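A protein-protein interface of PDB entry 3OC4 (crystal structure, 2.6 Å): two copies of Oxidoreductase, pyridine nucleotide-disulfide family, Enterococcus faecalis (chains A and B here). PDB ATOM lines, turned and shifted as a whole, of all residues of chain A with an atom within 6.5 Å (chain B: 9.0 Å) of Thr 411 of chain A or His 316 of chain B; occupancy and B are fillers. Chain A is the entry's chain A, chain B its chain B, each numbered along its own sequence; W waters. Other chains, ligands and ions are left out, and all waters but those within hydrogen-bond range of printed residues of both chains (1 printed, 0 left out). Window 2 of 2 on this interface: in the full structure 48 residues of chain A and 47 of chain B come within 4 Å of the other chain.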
ATOM      1  N   GLN A 380     -12.252   4.312 -24.429  1.00  0.00           N
ATOM      2  CA  GLN A 380     -11.878   3.036 -25.033  1.00  0.00           C
ATOM      3  C   GLN A 380     -12.510   2.831 -26.409  1.00  0.00           C
ATOM      4  O   GLN A 380     -12.675   1.699 -26.873  1.00  0.00           O
ATOM      5  CB  GLN A 380     -12.200   1.861 -24.096  1.00  0.00           C
ATOM      6  CG  GLN A 380     -11.228   1.803 -22.923  1.00  0.00           C
ATOM      7  CD  GLN A 380     -11.126   0.445 -22.239  1.00  0.00           C
ATOM      8  OE1 GLN A 380     -10.305   0.275 -21.343  1.00  0.00           O
ATOM      9  NE2 GLN A 380     -11.949  -0.524 -22.655  1.00  0.00           N
ATOM     10  N   GLN A 408     -17.291   1.384 -32.093  1.00  0.00           N
ATOM     11  CA  GLN A 408     -16.873   0.252 -31.275  1.00  0.00           C
ATOM     12  C   GLN A 408     -15.785   0.595 -30.272  1.00  0.00           C
ATOM     13  O   GLN A 408     -14.975   1.499 -30.490  1.00  0.00           O
ATOM     14  CB  GLN A 408     -16.371  -0.902 -32.143  1.00  0.00           C
ATOM     15  CG  GLN A 408     -17.440  -1.570 -32.950  1.00  0.00           C
ATOM     16  CD  GLN A 408     -17.101  -3.014 -33.256  1.00  0.00           C
ATOM     17  OE1 GLN A 408     -16.015  -3.321 -33.732  1.00  0.00           O
ATOM     18  NE2 GLN A 408     -18.037  -3.907 -32.982  1.00  0.00           N
ATOM     19  N   THR A 409     -15.781  -0.145 -29.165  1.00  0.00           N
ATOM     20  CA  THR A 409     -14.781   0.018 -28.121  1.00  0.00           C
ATOM     21  C   THR A 409     -13.799  -1.140 -28.270  1.00  0.00           C
ATOM     22  O   THR A 409     -14.001  -2.043 -29.096  1.00  0.00           O
ATOM     23  CB  THR A 409     -15.412  -0.039 -26.708  1.00  0.00           C
ATOM     24  OG1 THR A 409     -16.101  -1.286 -26.539  1.00  0.00           O
ATOM     25  CG2 THR A 409     -16.389   1.131 -26.502  1.00  0.00           C
ATOM     26  N   LEU A 410     -12.736  -1.121 -27.472  1.00  0.00           N
ATOM     27  CA  LEU A 410     -11.748  -2.189 -27.539  1.00  0.00           C
ATOM     28  C   LEU A 410     -12.458  -3.517 -27.278  1.00  0.00           C
ATOM     29  O   LEU A 410     -12.173  -4.539 -27.908  1.00  0.00           O
ATOM     30  CB  LEU A 410     -10.659  -1.949 -26.500  1.00  0.00           C
ATOM     31  CG  LEU A 410      -9.947  -0.599 -26.621  1.00  0.00           C
ATOM     32  CD1 LEU A 410      -8.937  -0.475 -25.505  1.00  0.00           C
ATOM     33  CD2 LEU A 410      -9.266  -0.481 -27.980  1.00  0.00           C
ATOM     34  N   THR A 411     -13.395  -3.469 -26.339  1.00  0.00           N
ATOM     35  CA  THR A 411     -14.202  -4.615 -25.941  1.00  0.00           C
ATOM     36  C   THR A 411     -15.071  -5.128 -27.102  1.00  0.00           C
ATOM     37  O   THR A 411     -15.220  -6.333 -27.280  1.00  0.00           O
ATOM     38  CB  THR A 411     -15.075  -4.228 -24.714  1.00  0.00           C
ATOM     39  OG1 THR A 411     -14.387  -4.608 -23.520  1.00  0.00           O
ATOM     40  CG2 THR A 411     -16.448  -4.882 -24.764  1.00  0.00           C
ATOM     41  N   ASP A 412     -15.627  -4.226 -27.902  1.00  0.00           N
ATOM     42  CA  ASP A 412     -16.457  -4.666 -29.025  1.00  0.00           C
ATOM     43  C   ASP A 412     -15.614  -5.321 -30.117  1.00  0.00           C
ATOM     44  O   ASP A 412     -15.953  -6.387 -30.621  1.00  0.00           O
ATOM     45  CB  ASP A 412     -17.229  -3.495 -29.652  1.00  0.00           C
ATOM     46  CG  ASP A 412     -18.118  -2.768 -28.664  1.00  0.00           C
ATOM     47  OD1 ASP A 412     -18.881  -3.421 -27.918  1.00  0.00           O
ATOM     48  OD2 ASP A 412     -18.058  -1.522 -28.652  1.00  0.00           O
ATOM     49  N   LEU A 413     -14.520  -4.661 -30.481  1.00  0.00           N
ATOM     50  CA  LEU A 413     -13.619  -5.134 -31.522  1.00  0.00           C
ATOM     51  C   LEU A 413     -13.050  -6.507 -31.171  1.00  0.00           C
ATOM     52  O   LEU A 413     -12.989  -7.414 -32.009  1.00  0.00           O
ATOM     53  CB  LEU A 413     -12.487  -4.110 -31.710  1.00  0.00           C
ATOM     54  CG  LEU A 413     -11.397  -4.412 -32.741  1.00  0.00           C
ATOM     55  CD1 LEU A 413     -12.047  -4.721 -34.071  1.00  0.00           C
ATOM     56  CD2 LEU A 413     -10.441  -3.235 -32.861  1.00  0.00           C
ATOM     57  N   LEU A 414     -12.639  -6.633 -29.914  1.00  0.00           N
ATOM     58  CA  LEU A 414     -12.075  -7.854 -29.350  1.00  0.00           C
ATOM     59  C   LEU A 414     -12.932  -9.107 -29.623  1.00  0.00           C
ATOM     60  O   LEU A 414     -12.398 -10.197 -29.879  1.00  0.00           O
ATOM     61  CB  LEU A 414     -11.910  -7.628 -27.846  1.00  0.00           C
ATOM     62  CG  LEU A 414     -11.550  -8.687 -26.806  1.00  0.00           C
ATOM     63  CD1 LEU A 414     -11.321  -7.976 -25.475  1.00  0.00           C
ATOM     64  CD2 LEU A 414     -12.659  -9.737 -26.658  1.00  0.00           C
ATOM     65  N   GLN A 415     -14.253  -8.953 -29.590  1.00  0.00           N
ATOM     66  CA  GLN A 415     -15.145 -10.094 -29.789  1.00  0.00           C
ATOM     67  C   GLN A 415     -16.067 -10.086 -31.005  1.00  0.00           C
ATOM     68  O   GLN A 415     -17.033 -10.853 -31.039  1.00  0.00           O
ATOM     69  CB  GLN A 415     -16.008 -10.313 -28.530  1.00  0.00           C
ATOM     70  CG  GLN A 415     -16.804  -9.085 -28.096  1.00  0.00           C
ATOM     71  CD  GLN A 415     -17.981  -9.408 -27.185  1.00  0.00           C
ATOM     72  OE1 GLN A 415     -18.475  -8.533 -26.484  1.00  0.00           O
ATOM     73  NE2 GLN A 415     -18.445 -10.657 -27.206  1.00  0.00           N
ATOM     74  N   LYS A 416     -15.794  -9.238 -31.991  1.00  0.00           N
ATOM     75  CA  LYS A 416     -16.635  -9.203 -33.188  1.00  0.00           C
ATOM     76  C   LYS A 416     -16.476 -10.520 -33.950  1.00  0.00           C
ATOM     77  O   LYS A 416     -15.454 -11.187 -33.842  1.00  0.00           O
ATOM     78  CB  LYS A 416     -16.224  -8.052 -34.110  1.00  0.00           C
ATOM     79  CG  LYS A 416     -14.850  -8.243 -34.762  1.00  0.00           C
ATOM     80  CD  LYS A 416     -14.462  -7.064 -35.622  1.00  0.00           C
ATOM     81  CE  LYS A 416     -13.129  -7.296 -36.317  1.00  0.00           C
ATOM     82  NZ  LYS A 416     -13.228  -8.439 -37.260  1.00  0.00           N
ATOM     83  N   GLY A 435      -7.691  -5.076 -30.847  1.00  0.00           N
ATOM     84  CA  GLY A 435      -8.583  -4.560 -29.827  1.00  0.00           C
ATOM     85  C   GLY A 435      -8.311  -5.240 -28.492  1.00  0.00           C
ATOM     86  O   GLY A 435      -8.247  -4.578 -27.452  1.00  0.00           O
ATOM     87  N   ALA A 436      -8.131  -6.560 -28.502  1.00  0.00           N
ATOM     88  CA  ALA A 436      -7.859  -7.281 -27.266  1.00  0.00           C
ATOM     89  C   ALA A 436      -6.552  -6.807 -26.619  1.00  0.00           C
ATOM     90  O   ALA A 436      -6.511  -6.521 -25.420  1.00  0.00           O
ATOM     91  CB  ALA A 436      -7.801  -8.777 -27.528  1.00  0.00           C
ATOM     92  N   TYR A 439      -7.024  -3.651 -24.932  1.00  0.00           N
ATOM     93  CA  TYR A 439      -7.842  -3.865 -23.739  1.00  0.00           C
ATOM     94  C   TYR A 439      -7.021  -4.396 -22.571  1.00  0.00           C
ATOM     95  O   TYR A 439      -7.106  -3.891 -21.455  1.00  0.00           O
ATOM     96  CB  TYR A 439      -8.967  -4.852 -24.048  1.00  0.00           C
ATOM     97  CG  TYR A 439      -9.834  -5.209 -22.870  1.00  0.00           C
ATOM     98  CD1 TYR A 439     -10.641  -4.256 -22.256  1.00  0.00           C
ATOM     99  CD2 TYR A 439      -9.872  -6.520 -22.384  1.00  0.00           C
ATOM    100  CE1 TYR A 439     -11.472  -4.590 -21.189  1.00  0.00           C
ATOM    101  CE2 TYR A 439     -10.699  -6.871 -21.314  1.00  0.00           C
ATOM    102  CZ  TYR A 439     -11.496  -5.901 -20.722  1.00  0.00           C
ATOM    103  OH  TYR A 439     -12.311  -6.241 -19.667  1.00  0.00           O
ATOM    104  N   LYS B  24      -6.430 -10.845 -16.869  1.00  0.00           N
ATOM    105  CA  LYS B  24      -7.247 -10.134 -15.902  1.00  0.00           C
ATOM    106  C   LYS B  24      -6.865 -10.381 -14.449  1.00  0.00           C
ATOM    107  O   LYS B  24      -7.058  -9.515 -13.597  1.00  0.00           O
ATOM    108  CB  LYS B  24      -8.718 -10.480 -16.100  1.00  0.00           C
ATOM    109  CG  LYS B  24      -9.623  -9.628 -15.236  1.00  0.00           C
ATOM    110  CD  LYS B  24     -11.065  -9.729 -15.659  1.00  0.00           C
ATOM    111  CE  LYS B  24     -11.890  -8.618 -15.019  1.00  0.00           C
ATOM    112  NZ  LYS B  24     -11.861  -8.705 -13.536  1.00  0.00           N
ATOM    113  N   ASP B 264     -26.463 -17.065 -19.661  1.00  0.00           N
ATOM    114  CA  ASP B 264     -27.016 -15.736 -19.868  1.00  0.00           C
ATOM    115  C   ASP B 264     -26.059 -14.992 -20.803  1.00  0.00           C
ATOM    116  O   ASP B 264     -25.124 -15.590 -21.337  1.00  0.00           O
ATOM    117  CB  ASP B 264     -27.155 -14.995 -18.538  1.00  0.00           C
ATOM    118  CG  ASP B 264     -25.816 -14.750 -17.845  1.00  0.00           C
ATOM    119  OD1 ASP B 264     -24.760 -15.163 -18.378  1.00  0.00           O
ATOM    120  OD2 ASP B 264     -25.825 -14.138 -16.753  1.00  0.00           O
ATOM    121  N   ALA B 265     -26.273 -13.694 -20.992  1.00  0.00           N
ATOM    122  CA  ALA B 265     -25.421 -12.921 -21.885  1.00  0.00           C
ATOM    123  C   ALA B 265     -23.966 -12.833 -21.430  1.00  0.00           C
ATOM    124  O   ALA B 265     -23.089 -12.500 -22.230  1.00  0.00           O
ATOM    125  CB  ALA B 265     -25.990 -11.521 -22.069  1.00  0.00           C
ATOM    126  N   TYR B 266     -23.704 -13.123 -20.159  1.00  0.00           N
ATOM    127  CA  TYR B 266     -22.338 -13.040 -19.648  1.00  0.00           C
ATOM    128  C   TYR B 266     -21.635 -14.388 -19.588  1.00  0.00           C
ATOM    129  O   TYR B 266     -20.550 -14.512 -19.032  1.00  0.00           O
ATOM    130  CB  TYR B 266     -22.332 -12.354 -18.278  1.00  0.00           C
ATOM    131  CG  TYR B 266     -22.953 -10.981 -18.344  1.00  0.00           C
ATOM    132  CD1 TYR B 266     -24.322 -10.797 -18.131  1.00  0.00           C
ATOM    133  CD2 TYR B 266     -22.190  -9.874 -18.724  1.00  0.00           C
ATOM    134  CE1 TYR B 266     -24.911  -9.548 -18.309  1.00  0.00           C
ATOM    135  CE2 TYR B 266     -22.761  -8.633 -18.905  1.00  0.00           C
ATOM    136  CZ  TYR B 266     -24.123  -8.472 -18.701  1.00  0.00           C
ATOM    137  OH  TYR B 266     -24.681  -7.233 -18.923  1.00  0.00           O
ATOM    138  N   LEU B 267     -22.274 -15.392 -20.168  1.00  0.00           N
ATOM    139  CA  LEU B 267     -21.731 -16.740 -20.247  1.00  0.00           C
ATOM    140  C   LEU B 267     -21.702 -17.540 -18.941  1.00  0.00           C
ATOM    141  O   LEU B 267     -20.917 -18.475 -18.793  1.00  0.00           O
ATOM    142  CB  LEU B 267     -20.335 -16.690 -20.880  1.00  0.00           C
ATOM    143  CG  LEU B 267     -20.336 -16.027 -22.261  1.00  0.00           C
ATOM    144  CD1 LEU B 267     -18.917 -15.808 -22.744  1.00  0.00           C
ATOM    145  CD2 LEU B 267     -21.120 -16.875 -23.235  1.00  0.00           C
ATOM    146  N   GLN B 268     -22.566 -17.181 -17.997  1.00  0.00           N
ATOM    147  CA  GLN B 268     -22.645 -17.914 -16.741  1.00  0.00           C
ATOM    148  C   GLN B 268     -23.786 -18.926 -16.866  1.00  0.00           C
ATOM    149  O   GLN B 268     -24.792 -18.656 -17.532  1.00  0.00           O
ATOM    150  CB  GLN B 268     -22.935 -16.973 -15.571  1.00  0.00           C
ATOM    151  CG  GLN B 268     -22.892 -17.682 -14.217  1.00  0.00           C
ATOM    152  CD  GLN B 268     -23.434 -16.844 -13.068  1.00  0.00           C
ATOM    153  OE1 GLN B 268     -23.025 -15.704 -12.864  1.00  0.00           O
ATOM    154  NE2 GLN B 268     -24.352 -17.417 -12.305  1.00  0.00           N
ATOM    155  N   ARG B 302     -13.830 -16.449 -28.971  1.00  0.00           N
ATOM    156  CA  ARG B 302     -14.444 -15.238 -28.463  1.00  0.00           C
ATOM    157  C   ARG B 302     -15.111 -15.444 -27.113  1.00  0.00           C
ATOM    158  O   ARG B 302     -14.890 -14.654 -26.192  1.00  0.00           O
ATOM    159  CB  ARG B 302     -15.415 -14.662 -29.500  1.00  0.00           C
ATOM    160  CG  ARG B 302     -14.687 -14.131 -30.738  1.00  0.00           C
ATOM    161  CD  ARG B 302     -15.628 -13.580 -31.793  1.00  0.00           C
ATOM    162  NE  ARG B 302     -16.668 -14.533 -32.147  1.00  0.00           N
ATOM    163  CZ  ARG B 302     -17.965 -14.322 -31.953  1.00  0.00           C
ATOM    164  NH1 ARG B 302     -18.375 -13.178 -31.413  1.00  0.00           N
ATOM    165  NH2 ARG B 302     -18.852 -15.254 -32.288  1.00  0.00           N
ATOM    166  N   THR B 303     -15.908 -16.493 -26.967  1.00  0.00           N
ATOM    167  CA  THR B 303     -16.545 -16.729 -25.671  1.00  0.00           C
ATOM    168  C   THR B 303     -15.478 -16.968 -24.573  1.00  0.00           C
ATOM    169  O   THR B 303     -15.667 -16.593 -23.412  1.00  0.00           O
ATOM    170  CB  THR B 303     -17.534 -17.924 -25.739  1.00  0.00           C
ATOM    171  OG1 THR B 303     -16.846 -19.106 -26.166  1.00  0.00           O
ATOM    172  CG2 THR B 303     -18.669 -17.623 -26.716  1.00  0.00           C
ATOM    173  N   LEU B 305     -12.446 -15.545 -24.382  1.00  0.00           N
ATOM    174  CA  LEU B 305     -11.830 -14.278 -24.000  1.00  0.00           C
ATOM    175  C   LEU B 305     -12.817 -13.386 -23.250  1.00  0.00           C
ATOM    176  O   LEU B 305     -12.422 -12.619 -22.376  1.00  0.00           O
ATOM    177  CB  LEU B 305     -11.325 -13.549 -25.239  1.00  0.00           C
ATOM    178  CG  LEU B 305     -10.267 -14.288 -26.052  1.00  0.00           C
ATOM    179  CD1 LEU B 305     -10.055 -13.575 -27.395  1.00  0.00           C
ATOM    180  CD2 LEU B 305      -8.973 -14.376 -25.242  1.00  0.00           C
ATOM    181  N   VAL B 306     -14.099 -13.493 -23.583  1.00  0.00           N
ATOM    182  CA  VAL B 306     -15.104 -12.678 -22.916  1.00  0.00           C
ATOM    183  C   VAL B 306     -15.483 -13.174 -21.518  1.00  0.00           C
ATOM    184  O   VAL B 306     -15.639 -12.364 -20.599  1.00  0.00           O
ATOM    185  CB  VAL B 306     -16.383 -12.553 -23.770  1.00  0.00           C
ATOM    186  CG1 VAL B 306     -17.475 -11.825 -22.988  1.00  0.00           C
ATOM    187  CG2 VAL B 306     -16.069 -11.785 -25.041  1.00  0.00           C
ATOM    188  N   VAL B 307     -15.624 -14.489 -21.348  1.00  0.00           N
ATOM    189  CA  VAL B 307     -16.000 -15.046 -20.050  1.00  0.00           C
ATOM    190  C   VAL B 307     -15.033 -14.648 -18.935  1.00  0.00           C
ATOM    191  O   VAL B 307     -15.447 -14.445 -17.800  1.00  0.00           O
ATOM    192  CB  VAL B 307     -16.102 -16.598 -20.095  1.00  0.00           C
ATOM    193  CG1 VAL B 307     -14.715 -17.224 -20.177  1.00  0.00           C
ATOM    194  CG2 VAL B 307     -16.856 -17.102 -18.869  1.00  0.00           C
ATOM    195  N   ALA B 308     -13.752 -14.521 -19.274  1.00  0.00           N
ATOM    196  CA  ALA B 308     -12.718 -14.155 -18.309  1.00  0.00           C
ATOM    197  C   ALA B 308     -12.962 -12.797 -17.656  1.00  0.00           C
ATOM    198  O   ALA B 308     -12.389 -12.496 -16.612  1.00  0.00           O
ATOM    199  CB  ALA B 308     -11.350 -14.162 -18.989  1.00  0.00           C
ATOM    200  N   ASN B 309     -13.808 -11.977 -18.267  1.00  0.00           N
ATOM    201  CA  ASN B 309     -14.101 -10.659 -17.717  1.00  0.00           C
ATOM    202  C   ASN B 309     -15.421 -10.611 -16.946  1.00  0.00           C
ATOM    203  O   ASN B 309     -15.811  -9.552 -16.454  1.00  0.00           O
ATOM    204  CB  ASN B 309     -14.119  -9.605 -18.834  1.00  0.00           C
ATOM    205  CG  ASN B 309     -12.779  -9.500 -19.566  1.00  0.00           C
ATOM    206  OD1 ASN B 309     -11.728  -9.320 -18.941  1.00  0.00           O
ATOM    207  ND2 ASN B 309     -12.814  -9.608 -20.897  1.00  0.00           N
ATOM    208  N   ASN B 310     -16.100 -11.755 -16.831  1.00  0.00           N
ATOM    209  CA  ASN B 310     -17.379 -11.806 -16.128  1.00  0.00           C
ATOM    210  C   ASN B 310     -17.432 -12.836 -15.015  1.00  0.00           C
ATOM    211  O   ASN B 310     -18.519 -13.272 -14.635  1.00  0.00           O
ATOM    212  CB  ASN B 310     -18.517 -12.101 -17.102  1.00  0.00           C
ATOM    213  CG  ASN B 310     -18.607 -11.087 -18.205  1.00  0.00           C
ATOM    214  OD1 ASN B 310     -18.378  -9.901 -17.982  1.00  0.00           O
ATOM    215  ND2 ASN B 310     -18.955 -11.538 -19.406  1.00  0.00           N
ATOM    216  N   LEU B 311     -16.271 -13.227 -14.496  1.00  0.00           N
ATOM    217  CA  LEU B 311     -16.215 -14.221 -13.430  1.00  0.00           C
ATOM    218  C   LEU B 311     -16.762 -13.680 -12.109  1.00  0.00           C
ATOM    219  O   LEU B 311     -17.279 -14.440 -11.292  1.00  0.00           O
ATOM    220  CB  LEU B 311     -14.780 -14.713 -13.241  1.00  0.00           C
ATOM    221  CG  LEU B 311     -14.123 -15.350 -14.473  1.00  0.00           C
ATOM    222  CD1 LEU B 311     -12.745 -15.874 -14.081  1.00  0.00           C
ATOM    223  CD2 LEU B 311     -15.012 -16.478 -15.041  1.00  0.00           C
ATOM    224  N   GLU B 313     -18.025  -9.672 -11.601  1.00  0.00           N
ATOM    225  CA  GLU B 313     -19.066  -8.730 -11.981  1.00  0.00           C
ATOM    226  C   GLU B 313     -19.384  -8.914 -13.457  1.00  0.00           C
ATOM    227  O   GLU B 313     -18.485  -9.168 -14.260  1.00  0.00           O
ATOM    228  CB  GLU B 313     -18.600  -7.296 -11.741  1.00  0.00           C
ATOM    229  CG  GLU B 313     -18.176  -7.020 -10.312  1.00  0.00           C
ATOM    230  CD  GLU B 313     -17.847  -5.555 -10.072  1.00  0.00           C
ATOM    231  OE1 GLU B 313     -16.846  -5.057 -10.641  1.00  0.00           O
ATOM    232  OE2 GLU B 313     -18.598  -4.899  -9.313  1.00  0.00           O
ATOM    233  N   LYS B 314     -20.663  -8.805 -13.807  1.00  0.00           N
ATOM    234  CA  LYS B 314     -21.088  -8.925 -15.199  1.00  0.00           C
ATOM    235  C   LYS B 314     -20.727  -7.598 -15.865  1.00  0.00           C
ATOM    236  O   LYS B 314     -21.497  -6.646 -15.807  1.00  0.00           O
ATOM    237  CB  LYS B 314     -22.603  -9.167 -15.285  1.00  0.00           C
ATOM    238  CG  LYS B 314     -23.085 -10.399 -14.522  1.00  0.00           C
ATOM    239  CD  LYS B 314     -22.210 -11.615 -14.812  1.00  0.00           C
ATOM    240  CE  LYS B 314     -22.745 -12.894 -14.167  1.00  0.00           C
ATOM    241  NZ  LYS B 314     -23.939 -13.473 -14.860  1.00  0.00           N
ATOM    242  N   THR B 315     -19.554  -7.546 -16.494  1.00  0.00           N
ATOM    243  CA  THR B 315     -19.057  -6.329 -17.135  1.00  0.00           C
ATOM    244  C   THR B 315     -19.202  -6.225 -18.657  1.00  0.00           C
ATOM    245  O   THR B 315     -19.426  -5.135 -19.185  1.00  0.00           O
ATOM    246  CB  THR B 315     -17.548  -6.102 -16.812  1.00  0.00           C
ATOM    247  OG1 THR B 315     -16.749  -7.021 -17.569  1.00  0.00           O
ATOM    248  CG2 THR B 315     -17.267  -6.326 -15.329  1.00  0.00           C
ATOM    249  N   HIS B 316     -19.060  -7.335 -19.373  1.00  0.00           N
ATOM    250  CA  HIS B 316     -19.159  -7.280 -20.826  1.00  0.00           C
ATOM    251  C   HIS B 316     -20.022  -8.374 -21.438  1.00  0.00           C
ATOM    252  O   HIS B 316     -19.675  -9.547 -21.387  1.00  0.00           O
ATOM    253  CB  HIS B 316     -17.755  -7.322 -21.441  1.00  0.00           C
ATOM    254  CG  HIS B 316     -16.887  -6.161 -21.049  1.00  0.00           C
ATOM    255  ND1 HIS B 316     -17.216  -4.851 -21.335  1.00  0.00           N
ATOM    256  CD2 HIS B 316     -15.704  -6.114 -20.387  1.00  0.00           C
ATOM    257  CE1 HIS B 316     -16.274  -4.049 -20.867  1.00  0.00           C
ATOM    258  NE2 HIS B 316     -15.345  -4.790 -20.287  1.00  0.00           N
ATOM    259  N   ARG B 317     -21.151  -7.977 -22.017  1.00  0.00           N
ATOM    260  CA  ARG B 317     -22.057  -8.920 -22.655  1.00  0.00           C
ATOM    261  C   ARG B 317     -21.426  -9.524 -23.904  1.00  0.00           C
ATOM    262  O   ARG B 317     -20.813  -8.818 -24.706  1.00  0.00           O
ATOM    263  CB  ARG B 317     -23.367  -8.227 -23.052  1.00  0.00           C
ATOM    264  CG  ARG B 317     -24.371  -8.077 -21.922  1.00  0.00           C
ATOM    265  CD  ARG B 317     -25.681  -7.431 -22.386  1.00  0.00           C
ATOM    266  NE  ARG B 317     -26.292  -8.161 -23.496  1.00  0.00           N
ATOM    267  CZ  ARG B 317     -27.494  -8.733 -23.451  1.00  0.00           C
ATOM    268  NH1 ARG B 317     -28.226  -8.665 -22.341  1.00  0.00           N
ATOM    269  NH2 ARG B 317     -27.967  -9.375 -24.517  1.00  0.00           N
ATOM    270  N   PHE B 318     -21.569 -10.835 -24.062  1.00  0.00           N
ATOM    271  CA  PHE B 318     -21.039 -11.505 -25.242  1.00  0.00           C
ATOM    272  C   PHE B 318     -21.968 -11.095 -26.381  1.00  0.00           C
ATOM    273  O   PHE B 318     -23.192 -11.223 -26.270  1.00  0.00           O
ATOM    274  CB  PHE B 318     -21.047 -13.025 -25.054  1.00  0.00           C
ATOM    275  CG  PHE B 318     -20.676 -13.791 -26.285  1.00  0.00           C
ATOM    276  CD1 PHE B 318     -19.457 -13.576 -26.916  1.00  0.00           C
ATOM    277  CD2 PHE B 318     -21.550 -14.731 -26.820  1.00  0.00           C
ATOM    278  CE1 PHE B 318     -19.114 -14.283 -28.065  1.00  0.00           C
ATOM    279  CE2 PHE B 318     -21.214 -15.438 -27.960  1.00  0.00           C
ATOM    280  CZ  PHE B 318     -19.992 -15.211 -28.588  1.00  0.00           C
ATOM    281  N   ILE B 319     -21.379 -10.590 -27.463  1.00  0.00           N
ATOM    282  CA  ILE B 319     -22.138 -10.119 -28.610  1.00  0.00           C
ATOM    283  C   ILE B 319     -22.953 -11.203 -29.299  1.00  0.00           C
ATOM    284  O   ILE B 319     -24.012 -10.925 -29.847  1.00  0.00           O
ATOM    285  CB  ILE B 319     -21.198  -9.458 -29.652  1.00  0.00           C
ATOM    286  CG1 ILE B 319     -22.019  -8.781 -30.752  1.00  0.00           C
ATOM    287  CG2 ILE B 319     -20.275 -10.498 -30.249  1.00  0.00           C
ATOM    288  CD1 ILE B 319     -22.950  -7.677 -30.253  1.00  0.00           C
ATOM    289  N   GLY B 320     -22.466 -12.437 -29.265  1.00  0.00           N
ATOM    290  CA  GLY B 320     -23.187 -13.516 -29.918  1.00  0.00           C
ATOM    291  C   GLY B 320     -22.459 -14.012 -31.156  1.00  0.00           C
ATOM    292  O   GLY B 320     -21.266 -13.772 -31.331  1.00  0.00           O
HETATM  293  O   HOH W   1     -13.757  -7.434 -16.939  1.00  0.00           O
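Water W1 lies within hydrogen-bond range of O of Asn 309 of chain B (3.0 Å), OG1 of Thr 315 of chain B (3.1 Å) and OH of Tyr 439 of chain A (3.3 Å).
Of the 23 printed residues of chain B, 7 touch a printed residue of chain A.
Of the 13 printed residues of chain A, 4 touch a printed residue of chain B.
Among the printed residues, 9 pairs touch across the chains.
Among the printed residues, no Asp or Glu carboxylate lies within 4 Å of a Lys or Arg side-chain nitrogen of the other chain.
No position is printed for both chains.
OG1 of Thr 411 of chain A sits close to NE2 of His 316 of chain B (3.4 Å).
The guanidinium group (NH1) of Arg 302 of chain B is in hydrogen-bond range of the backbone carbonyl oxygen (O) of Gln 415 of chain A (2.7 Å).
OE1 of Gln 415 of chain A sits close to O of Arg 317 of chain B (3.0 Å).
The side-chain amide nitrogen of Gln 415 of chain A sits close to the backbone NH of Ile 319 of chain B (2.9 Å).
The side-chain hydroxyl of Tyr 439 of chain A sits at hydrogen-bond distance from the side-chain amide oxygen of Asn 309 of chain B, at 3.2 Å.
NE2 of His 316 of chain B lies within hydrogen-bond range of OH of Tyr 439 of chain A (3.4 Å).
Among the printed residues, pairs that only touch across the chains: Gln 415 of chain A with Val 306 of chain B (3.4 Å), Gln 415 of chain A with Phe 318 of chain B (3.1 Å) and Lys 416 of chain A with Arg 302 of chain B (3.2 Å).
OG1 of Thr 409 of chain A sits close to N of Thr 411 of chain A (3.5 Å).
The backbone NH of Phe 318 of chain B is in hydrogen-bond range of the backbone carbonyl oxygen of Ala 265 of chain B (2.9 Å).
O of Gly 320 of chain B lies within hydrogen-bond range of NH1 of Arg 302 of chain B (3.0 Å).
The backbone carbonyl oxygen (O) of Leu 305 of chain B is in hydrogen-bond range of the side-chain amide nitrogen (ND2) of Asn 309 of chain B (3.4 Å).
The side-chain hydroxyl (OG1) of Thr 315 of chain B is in hydrogen-bond range of the backbone carbonyl oxygen (O) of Asn 309 of chain B (2.9 Å).
The backbone carbonyl oxygen (O) of His 316 of chain B lies within hydrogen-bond range of the side-chain amide nitrogen (ND2) of Asn 310 of chain B (2.9 Å).
Thr 411 of chain A touches just one residue of chain B: His 316 (3.3 Å).
Of the printed residues of chain B, Lys 416 of chain A touches Arg 302.
Printed residues of chain A within 4 Å of Val 306 of chain B: Gln 415 (3.4 Å).
Of the printed residues of chain A, Arg 302 of chain B touches Gln 415 and Lys 416.
Of the printed residues of chain A, Phe 318 of chain B touches Gln 415.
Asn 310 of chain B touches none of the printed residues of chain A.
The nearest printed residue of chain B that does not touch Thr 411 of chain A is Asn 309 of chain B (5.9 Å).
The nearest printed residue of chain A that does not touch Arg 302 of chain B is Leu 414 of chain A (4.6 Å).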
